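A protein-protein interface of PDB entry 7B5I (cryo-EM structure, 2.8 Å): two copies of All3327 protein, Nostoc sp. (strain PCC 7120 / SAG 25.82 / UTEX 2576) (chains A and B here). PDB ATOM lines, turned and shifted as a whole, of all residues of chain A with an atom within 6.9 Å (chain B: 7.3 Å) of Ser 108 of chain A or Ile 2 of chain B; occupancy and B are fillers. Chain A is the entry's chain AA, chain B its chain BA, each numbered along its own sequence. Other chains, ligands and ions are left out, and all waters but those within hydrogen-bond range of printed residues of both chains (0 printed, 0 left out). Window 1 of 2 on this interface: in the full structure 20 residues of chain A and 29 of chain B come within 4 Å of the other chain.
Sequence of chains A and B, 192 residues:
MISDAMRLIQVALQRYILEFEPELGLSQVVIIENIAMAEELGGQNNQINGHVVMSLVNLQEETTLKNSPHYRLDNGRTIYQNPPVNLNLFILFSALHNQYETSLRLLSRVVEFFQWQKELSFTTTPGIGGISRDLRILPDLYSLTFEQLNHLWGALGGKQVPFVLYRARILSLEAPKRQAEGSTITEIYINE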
ATOM      1  N   TYR A  16     -24.686   4.975  10.772  1.00  0.00           N
ATOM      2  CA  TYR A  16     -23.594   5.748  10.180  1.00  0.00           C
ATOM      3  C   TYR A  16     -22.700   6.365  11.250  1.00  0.00           C
ATOM      4  O   TYR A  16     -21.470   6.189  11.241  1.00  0.00           O
ATOM      5  CB  TYR A  16     -24.169   6.832   9.273  1.00  0.00           C
ATOM      6  CG  TYR A  16     -23.145   7.723   8.612  1.00  0.00           C
ATOM      7  CD1 TYR A  16     -22.557   7.361   7.413  1.00  0.00           C
ATOM      8  CD2 TYR A  16     -22.787   8.936   9.177  1.00  0.00           C
ATOM      9  CE1 TYR A  16     -21.633   8.177   6.801  1.00  0.00           C
ATOM     10  CE2 TYR A  16     -21.862   9.756   8.573  1.00  0.00           C
ATOM     11  CZ  TYR A  16     -21.291   9.372   7.387  1.00  0.00           C
ATOM     12  OH  TYR A  16     -20.371  10.189   6.786  1.00  0.00           O
ATOM     13  N   THR A 102     -18.517  18.551  20.872  1.00  0.00           N
ATOM     14  CA  THR A 102     -19.137  17.306  20.446  1.00  0.00           C
ATOM     15  C   THR A 102     -20.377  17.581  19.609  1.00  0.00           C
ATOM     16  O   THR A 102     -20.640  16.886  18.619  1.00  0.00           O
ATOM     17  CB  THR A 102     -19.488  16.466  21.670  1.00  0.00           C
ATOM     18  OG1 THR A 102     -18.307  16.254  22.449  1.00  0.00           O
ATOM     19  CG2 THR A 102     -20.055  15.129  21.253  1.00  0.00           C
ATOM     20  N   SER A 103     -21.140  18.607  19.986  1.00  0.00           N
ATOM     21  CA  SER A 103     -22.328  18.969  19.228  1.00  0.00           C
ATOM     22  C   SER A 103     -21.972  19.339  17.796  1.00  0.00           C
ATOM     23  O   SER A 103     -22.651  18.924  16.850  1.00  0.00           O
ATOM     24  CB  SER A 103     -23.046  20.123  19.920  1.00  0.00           C
ATOM     25  OG  SER A 103     -23.540  19.729  21.186  1.00  0.00           O
ATOM     26  N   LEU A 104     -20.893  20.101  17.614  1.00  0.00           N
ATOM     27  CA  LEU A 104     -20.504  20.523  16.274  1.00  0.00           C
ATOM     28  C   LEU A 104     -20.007  19.344  15.445  1.00  0.00           C
ATOM     29  O   LEU A 104     -20.321  19.239  14.250  1.00  0.00           O
ATOM     30  CB  LEU A 104     -19.439  21.611  16.370  1.00  0.00           C
ATOM     31  CG  LEU A 104     -19.878  22.864  17.127  1.00  0.00           C
ATOM     32  CD1 LEU A 104     -18.704  23.806  17.351  1.00  0.00           C
ATOM     33  CD2 LEU A 104     -21.002  23.571  16.392  1.00  0.00           C
ATOM     34  N   ARG A 105     -19.238  18.445  16.062  1.00  0.00           N
ATOM     35  CA  ARG A 105     -18.798  17.255  15.338  1.00  0.00           C
ATOM     36  C   ARG A 105     -19.987  16.419  14.873  1.00  0.00           C
ATOM     37  O   ARG A 105     -20.045  15.982  13.712  1.00  0.00           O
ATOM     38  CB  ARG A 105     -17.866  16.418  16.209  1.00  0.00           C
ATOM     39  CG  ARG A 105     -16.436  16.910  16.216  1.00  0.00           C
ATOM     40  CD  ARG A 105     -15.454  15.774  16.432  1.00  0.00           C
ATOM     41  NE  ARG A 105     -15.714  15.048  17.669  1.00  0.00           N
ATOM     42  CZ  ARG A 105     -15.302  15.446  18.867  1.00  0.00           C
ATOM     43  NH1 ARG A 105     -14.615  16.573  18.994  1.00  0.00           N
ATOM     44  NH2 ARG A 105     -15.581  14.719  19.940  1.00  0.00           N
ATOM     45  N   LEU A 106     -20.956  16.205  15.761  1.00  0.00           N
ATOM     46  CA  LEU A 106     -22.101  15.388  15.390  1.00  0.00           C
ATOM     47  C   LEU A 106     -22.969  16.073  14.341  1.00  0.00           C
ATOM     48  O   LEU A 106     -23.524  15.397  13.467  1.00  0.00           O
ATOM     49  CB  LEU A 106     -22.913  15.043  16.631  1.00  0.00           C
ATOM     50  CG  LEU A 106     -22.131  14.218  17.650  1.00  0.00           C
ATOM     51  CD1 LEU A 106     -23.021  13.825  18.810  1.00  0.00           C
ATOM     52  CD2 LEU A 106     -21.523  13.001  16.997  1.00  0.00           C
ATOM     53  N   LEU A 107     -23.086  17.401  14.391  1.00  0.00           N
ATOM     54  CA  LEU A 107     -23.793  18.106  13.328  1.00  0.00           C
ATOM     55  C   LEU A 107     -23.109  17.915  11.982  1.00  0.00           C
ATOM     56  O   LEU A 107     -23.777  17.700  10.961  1.00  0.00           O
ATOM     57  CB  LEU A 107     -23.893  19.594  13.645  1.00  0.00           C
ATOM     58  CG  LEU A 107     -25.153  20.092  14.341  1.00  0.00           C
ATOM     59  CD1 LEU A 107     -25.204  21.601  14.225  1.00  0.00           C
ATOM     60  CD2 LEU A 107     -26.393  19.457  13.743  1.00  0.00           C
ATOM     61  N   SER A 108     -21.779  18.016  11.956  1.00  0.00           N
ATOM     62  CA  SER A 108     -21.060  17.804  10.705  1.00  0.00           C
ATOM     63  C   SER A 108     -21.328  16.411  10.155  1.00  0.00           C
ATOM     64  O   SER A 108     -21.537  16.235   8.944  1.00  0.00           O
ATOM     65  CB  SER A 108     -19.567  18.022  10.921  1.00  0.00           C
ATOM     66  OG  SER A 108     -19.308  19.370  11.259  1.00  0.00           O
ATOM     67  N   ARG A 109     -21.355  15.411  11.036  1.00  0.00           N
ATOM     68  CA  ARG A 109     -21.583  14.053  10.556  1.00  0.00           C
ATOM     69  C   ARG A 109     -23.013  13.850  10.072  1.00  0.00           C
ATOM     70  O   ARG A 109     -23.234  13.121   9.101  1.00  0.00           O
ATOM     71  CB  ARG A 109     -21.219  13.044  11.638  1.00  0.00           C
ATOM     72  CG  ARG A 109     -19.727  12.990  11.860  1.00  0.00           C
ATOM     73  CD  ARG A 109     -19.262  11.639  12.328  1.00  0.00           C
ATOM     74  NE  ARG A 109     -17.839  11.641  12.647  1.00  0.00           N
ATOM     75  CZ  ARG A 109     -16.866  11.669  11.742  1.00  0.00           C
ATOM     76  NH1 ARG A 109     -17.155  11.700  10.450  1.00  0.00           N
ATOM     77  NH2 ARG A 109     -15.601  11.667  12.130  1.00  0.00           N
ATOM     78  N   VAL A 110     -23.989  14.502  10.707  1.00  0.00           N
ATOM     79  CA  VAL A 110     -25.364  14.451  10.211  1.00  0.00           C
ATOM     80  C   VAL A 110     -25.439  15.027   8.801  1.00  0.00           C
ATOM     81  O   VAL A 110     -26.047  14.439   7.890  1.00  0.00           O
ATOM     82  CB  VAL A 110     -26.304  15.201  11.170  1.00  0.00           C
ATOM     83  CG1 VAL A 110     -27.665  15.407  10.534  1.00  0.00           C
ATOM     84  CG2 VAL A 110     -26.438  14.448  12.471  1.00  0.00           C
ATOM     85  N   VAL A 111     -24.821  16.192   8.606  1.00  0.00           N
ATOM     86  CA  VAL A 111     -24.856  16.841   7.301  1.00  0.00           C
ATOM     87  C   VAL A 111     -24.238  15.945   6.238  1.00  0.00           C
ATOM     88  O   VAL A 111     -24.790  15.785   5.144  1.00  0.00           O
ATOM     89  CB  VAL A 111     -24.158  18.210   7.365  1.00  0.00           C
ATOM     90  CG1 VAL A 111     -23.978  18.774   5.970  1.00  0.00           C
ATOM     91  CG2 VAL A 111     -24.960  19.162   8.221  1.00  0.00           C
ATOM     92  N   GLU A 112     -23.095  15.328   6.539  1.00  0.00           N
ATOM     93  CA  GLU A 112     -22.466  14.514   5.502  1.00  0.00           C
ATOM     94  C   GLU A 112     -23.207  13.198   5.275  1.00  0.00           C
ATOM     95  O   GLU A 112     -23.208  12.677   4.150  1.00  0.00           O
ATOM     96  CB  GLU A 112     -20.997  14.268   5.828  1.00  0.00           C
ATOM     97  CG  GLU A 112     -20.738  13.368   6.999  1.00  0.00           C
ATOM     98  CD  GLU A 112     -19.281  13.362   7.379  1.00  0.00           C
ATOM     99  OE1 GLU A 112     -18.657  14.441   7.325  1.00  0.00           O
ATOM    100  OE2 GLU A 112     -18.757  12.286   7.726  1.00  0.00           O
ATOM    101  N   PHE A 113     -23.862  12.653   6.304  1.00  0.00           N
ATOM    102  CA  PHE A 113     -24.696  11.480   6.075  1.00  0.00           C
ATOM    103  C   PHE A 113     -25.811  11.793   5.094  1.00  0.00           C
ATOM    104  O   PHE A 113     -26.094  10.998   4.191  1.00  0.00           O
ATOM    105  CB  PHE A 113     -25.294  10.957   7.377  1.00  0.00           C
ATOM    106  CG  PHE A 113     -26.379   9.944   7.157  1.00  0.00           C
ATOM    107  CD1 PHE A 113     -26.069   8.648   6.795  1.00  0.00           C
ATOM    108  CD2 PHE A 113     -27.712  10.295   7.278  1.00  0.00           C
ATOM    109  CE1 PHE A 113     -27.061   7.720   6.576  1.00  0.00           C
ATOM    110  CE2 PHE A 113     -28.709   9.368   7.057  1.00  0.00           C
ATOM    111  CZ  PHE A 113     -28.381   8.080   6.706  1.00  0.00           C
ATOM    112  N   MET B   1     -14.725  19.225   9.268  1.00  0.00           N
ATOM    113  CA  MET B   1     -15.658  19.405  10.369  1.00  0.00           C
ATOM    114  C   MET B   1     -15.852  20.876  10.696  1.00  0.00           C
ATOM    115  O   MET B   1     -15.172  21.738  10.150  1.00  0.00           O
ATOM    116  CB  MET B   1     -15.176  18.663  11.612  1.00  0.00           C
ATOM    117  CG  MET B   1     -14.765  17.230  11.359  1.00  0.00           C
ATOM    118  SD  MET B   1     -16.157  16.194  10.878  1.00  0.00           S
ATOM    119  CE  MET B   1     -16.081  14.923  12.136  1.00  0.00           C
ATOM    120  N   ILE B   2     -16.787  21.153  11.596  1.00  0.00           N
ATOM    121  CA  ILE B   2     -17.058  22.525  11.998  1.00  0.00           C
ATOM    122  C   ILE B   2     -16.191  22.948  13.180  1.00  0.00           C
ATOM    123  O   ILE B   2     -15.933  24.143  13.361  1.00  0.00           O
ATOM    124  CB  ILE B   2     -18.554  22.688  12.307  1.00  0.00           C
ATOM    125  CG1 ILE B   2     -19.370  22.342  11.066  1.00  0.00           C
ATOM    126  CG2 ILE B   2     -18.875  24.101  12.743  1.00  0.00           C
ATOM    127  CD1 ILE B   2     -20.853  22.434  11.271  1.00  0.00           C
ATOM    128  N   SER B   3     -15.706  21.993  13.972  1.00  0.00           N
ATOM    129  CA  SER B   3     -14.892  22.332  15.133  1.00  0.00           C
ATOM    130  C   SER B   3     -13.509  22.846  14.759  1.00  0.00           C
ATOM    131  O   SER B   3     -12.923  23.623  15.521  1.00  0.00           O
ATOM    132  CB  SER B   3     -14.756  21.109  16.036  1.00  0.00           C
ATOM    133  OG  SER B   3     -15.769  21.086  17.021  1.00  0.00           O
ATOM    134  N   ASP B   4     -12.991  22.468  13.592  1.00  0.00           N
ATOM    135  CA  ASP B   4     -11.616  22.820  13.265  1.00  0.00           C
ATOM    136  C   ASP B   4     -11.488  24.290  12.897  1.00  0.00           C
ATOM    137  O   ASP B   4     -10.520  24.950  13.294  1.00  0.00           O
ATOM    138  CB  ASP B   4     -11.105  21.940  12.129  1.00  0.00           C
ATOM    139  CG  ASP B   4     -11.103  20.472  12.490  1.00  0.00           C
ATOM    140  OD1 ASP B   4     -10.313  20.073  13.368  1.00  0.00           O
ATOM    141  OD2 ASP B   4     -11.887  19.711  11.888  1.00  0.00           O
ATOM    142  N   ALA B   5     -12.463  24.823  12.163  1.00  0.00           N
ATOM    143  CA  ALA B   5     -12.433  26.238  11.818  1.00  0.00           C
ATOM    144  C   ALA B   5     -12.520  27.108  13.063  1.00  0.00           C
ATOM    145  O   ALA B   5     -11.774  28.089  13.203  1.00  0.00           O
ATOM    146  CB  ALA B   5     -13.576  26.559  10.860  1.00  0.00           C
ATOM    147  N   MET B   6     -13.412  26.756  13.987  1.00  0.00           N
ATOM    148  CA  MET B   6     -13.550  27.557  15.191  1.00  0.00           C
ATOM    149  C   MET B   6     -12.337  27.415  16.095  1.00  0.00           C
ATOM    150  O   MET B   6     -11.941  28.390  16.741  1.00  0.00           O
ATOM    151  CB  MET B   6     -14.839  27.181  15.921  1.00  0.00           C
ATOM    152  CG  MET B   6     -16.084  27.551  15.129  1.00  0.00           C
ATOM    153  SD  MET B   6     -17.640  27.119  15.922  1.00  0.00           S
ATOM    154  CE  MET B   6     -17.879  28.535  16.986  1.00  0.00           C
ATOM    155  N   ARG B   7     -11.696  26.246  16.118  1.00  0.00           N
ATOM    156  CA  ARG B   7     -10.461  26.135  16.889  1.00  0.00           C
ATOM    157  C   ARG B   7      -9.353  26.988  16.287  1.00  0.00           C
ATOM    158  O   ARG B   7      -8.589  27.630  17.020  1.00  0.00           O
ATOM    159  CB  ARG B   7     -10.024  24.680  16.987  1.00  0.00           C
ATOM    160  CG  ARG B   7     -10.598  23.959  18.178  1.00  0.00           C
ATOM    161  CD  ARG B   7      -9.803  22.714  18.470  1.00  0.00           C
ATOM    162  NE  ARG B   7     -10.077  21.669  17.491  1.00  0.00           N
ATOM    163  CZ  ARG B   7     -10.978  20.707  17.663  1.00  0.00           C
ATOM    164  NH1 ARG B   7     -11.690  20.654  18.780  1.00  0.00           N
ATOM    165  NH2 ARG B   7     -11.165  19.797  16.719  1.00  0.00           N
ATOM    166  N   LEU B  56     -21.912  29.864  17.229  1.00  0.00           N
ATOM    167  CA  LEU B  56     -22.451  29.632  15.895  1.00  0.00           C
ATOM    168  C   LEU B  56     -23.949  29.902  15.926  1.00  0.00           C
ATOM    169  O   LEU B  56     -24.671  29.285  16.713  1.00  0.00           O
ATOM    170  CB  LEU B  56     -22.174  28.200  15.445  1.00  0.00           C
ATOM    171  CG  LEU B  56     -22.761  27.786  14.099  1.00  0.00           C
ATOM    172  CD1 LEU B  56     -21.997  28.429  12.965  1.00  0.00           C
ATOM    173  CD2 LEU B  56     -22.756  26.286  13.957  1.00  0.00           C
ATOM    174  N   LEU B  59     -26.462  28.838   9.626  1.00  0.00           N
ATOM    175  CA  LEU B  59     -25.752  27.955   8.706  1.00  0.00           C
ATOM    176  C   LEU B  59     -26.488  27.985   7.376  1.00  0.00           C
ATOM    177  O   LEU B  59     -27.608  27.481   7.283  1.00  0.00           O
ATOM    178  CB  LEU B  59     -25.687  26.542   9.272  1.00  0.00           C
ATOM    179  CG  LEU B  59     -24.581  25.612   8.796  1.00  0.00           C
ATOM    180  CD1 LEU B  59     -23.238  26.184   9.189  1.00  0.00           C
ATOM    181  CD2 LEU B  59     -24.767  24.249   9.417  1.00  0.00           C
ATOM    182  N   LEU B  87     -20.941  25.533   2.735  1.00  0.00           N
ATOM    183  CA  LEU B  87     -21.685  26.265   3.745  1.00  0.00           C
ATOM    184  C   LEU B  87     -20.996  27.572   4.106  1.00  0.00           C
ATOM    185  O   LEU B  87     -19.763  27.667   4.114  1.00  0.00           O
ATOM    186  CB  LEU B  87     -21.855  25.428   5.013  1.00  0.00           C
ATOM    187  CG  LEU B  87     -22.555  24.082   4.857  1.00  0.00           C
ATOM    188  CD1 LEU B  87     -22.245  23.206   6.046  1.00  0.00           C
ATOM    189  CD2 LEU B  87     -24.052  24.275   4.711  1.00  0.00           C
ATOM    190  N   LEU B  89     -20.847  30.289   7.353  1.00  0.00           N
ATOM    191  CA  LEU B  89     -20.998  30.227   8.798  1.00  0.00           C
ATOM    192  C   LEU B  89     -21.154  31.626   9.374  1.00  0.00           C
ATOM    193  O   LEU B  89     -20.541  32.581   8.895  1.00  0.00           O
ATOM    194  CB  LEU B  89     -19.802  29.539   9.450  1.00  0.00           C
ATOM    195  CG  LEU B  89     -19.822  28.016   9.548  1.00  0.00           C
ATOM    196  CD1 LEU B  89     -19.760  27.380   8.180  1.00  0.00           C
ATOM    197  CD2 LEU B  89     -18.666  27.544  10.401  1.00  0.00           C
ATOM    198  N   LEU B 171     -17.055  26.508   3.756  1.00  0.00           N
ATOM    199  CA  LEU B 171     -16.660  25.271   4.414  1.00  0.00           C
ATOM    200  C   LEU B 171     -17.366  24.120   3.719  1.00  0.00           C
ATOM    201  O   LEU B 171     -18.587  24.150   3.565  1.00  0.00           O
ATOM    202  CB  LEU B 171     -17.007  25.302   5.901  1.00  0.00           C
ATOM    203  CG  LEU B 171     -16.483  24.150   6.746  1.00  0.00           C
ATOM    204  CD1 LEU B 171     -15.733  24.708   7.935  1.00  0.00           C
ATOM    205  CD2 LEU B 171     -17.634  23.275   7.209  1.00  0.00           C
ATOM    206  N   LEU B 173     -18.278  20.038   3.090  1.00  0.00           N
ATOM    207  CA  LEU B 173     -18.515  18.790   3.794  1.00  0.00           C
ATOM    208  C   LEU B 173     -18.937  17.712   2.808  1.00  0.00           C
ATOM    209  O   LEU B 173     -19.693  17.979   1.868  1.00  0.00           O
ATOM    210  CB  LEU B 173     -19.597  18.950   4.861  1.00  0.00           C
ATOM    211  CG  LEU B 173     -19.372  19.950   5.989  1.00  0.00           C
ATOM    212  CD1 LEU B 173     -20.603  20.005   6.860  1.00  0.00           C
ATOM    213  CD2 LEU B 173     -18.165  19.552   6.812  1.00  0.00           C
ATOM    214  N   GLU B 174     -18.449  16.494   3.031  1.00  0.00           N
ATOM    215  CA  GLU B 174     -18.846  15.342   2.234  1.00  0.00           C
ATOM    216  C   GLU B 174     -18.396  14.071   2.935  1.00  0.00           C
ATOM    217  O   GLU B 174     -17.569  14.103   3.848  1.00  0.00           O
ATOM    218  CB  GLU B 174     -18.263  15.404   0.825  1.00  0.00           C
ATOM    219  CG  GLU B 174     -16.765  15.354   0.782  1.00  0.00           C
ATOM    220  CD  GLU B 174     -16.249  15.342  -0.630  1.00  0.00           C
ATOM    221  OE1 GLU B 174     -17.079  15.286  -1.556  1.00  0.00           O
ATOM    222  OE2 GLU B 174     -15.017  15.393  -0.817  1.00  0.00           O
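No position is printed for both chains.
Of the 7 pairs that touch across the chains among the printed residues, none has its exchanged pair printed and touching as well.
Of the 14 printed residues of chain B, 6 touch a printed residue of chain A.
Hydrophobic or aromatic side chains of chain B that line the printed part of chain A: Met 1, Ile 2, Met 6 and Leu 173.
OH of Tyr 16 of chain A lies within hydrogen-bond range of OE2 of Glu 112 of chain A, at 2.8 Å.
OG of Ser 108 of chain A lies within hydrogen-bond range of O of Leu 104 of chain A, at 3.2 Å.
NH1 of Arg 109 of chain A lies within salt-bridge range of OE2 of Glu 112 of chain A (3.2 Å).
Among the printed residues, pairs that only touch across the chains: Arg 109 of chain A with Met 1 of chain B (3.3 Å), Glu 112 of chain A with Glu 174 of chain B (3.7 Å), Val 111 of chain A with Leu 173 of chain B (3.7 Å), Ser 108 of chain A with Met 1 of chain B (3.8 Å), Leu 104 of chain A with Met 6 of chain B (3.8 Å) and Leu 104 of chain A with Ser 3 of chain B (3.8 Å).
Printed residues of chain B within 4 Å of Ser 108 of chain A: Met 1 (3.8 Å) and Ile 2 (3.0 Å).
Printed residues of chain A within 4 Å of Leu 173 of chain B: Val 111.
Of the printed residues of chain B, Glu 112 of chain A touches Glu 174.
Printed residues of chain B within 4 Å of Val 111 of chain A: Leu 173 (3.7 Å).
Leu 56 of chain B touches none of the printed residues of chain A.
The nearest printed residue of chain A that does not touch Ser 3 of chain B is Arg 105 of chain A (4.3 Å).
The side-chain hydroxyl of Ser 108 of chain A sits close to the backbone NH of Ile 2 of chain B, at 3.1 Å.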
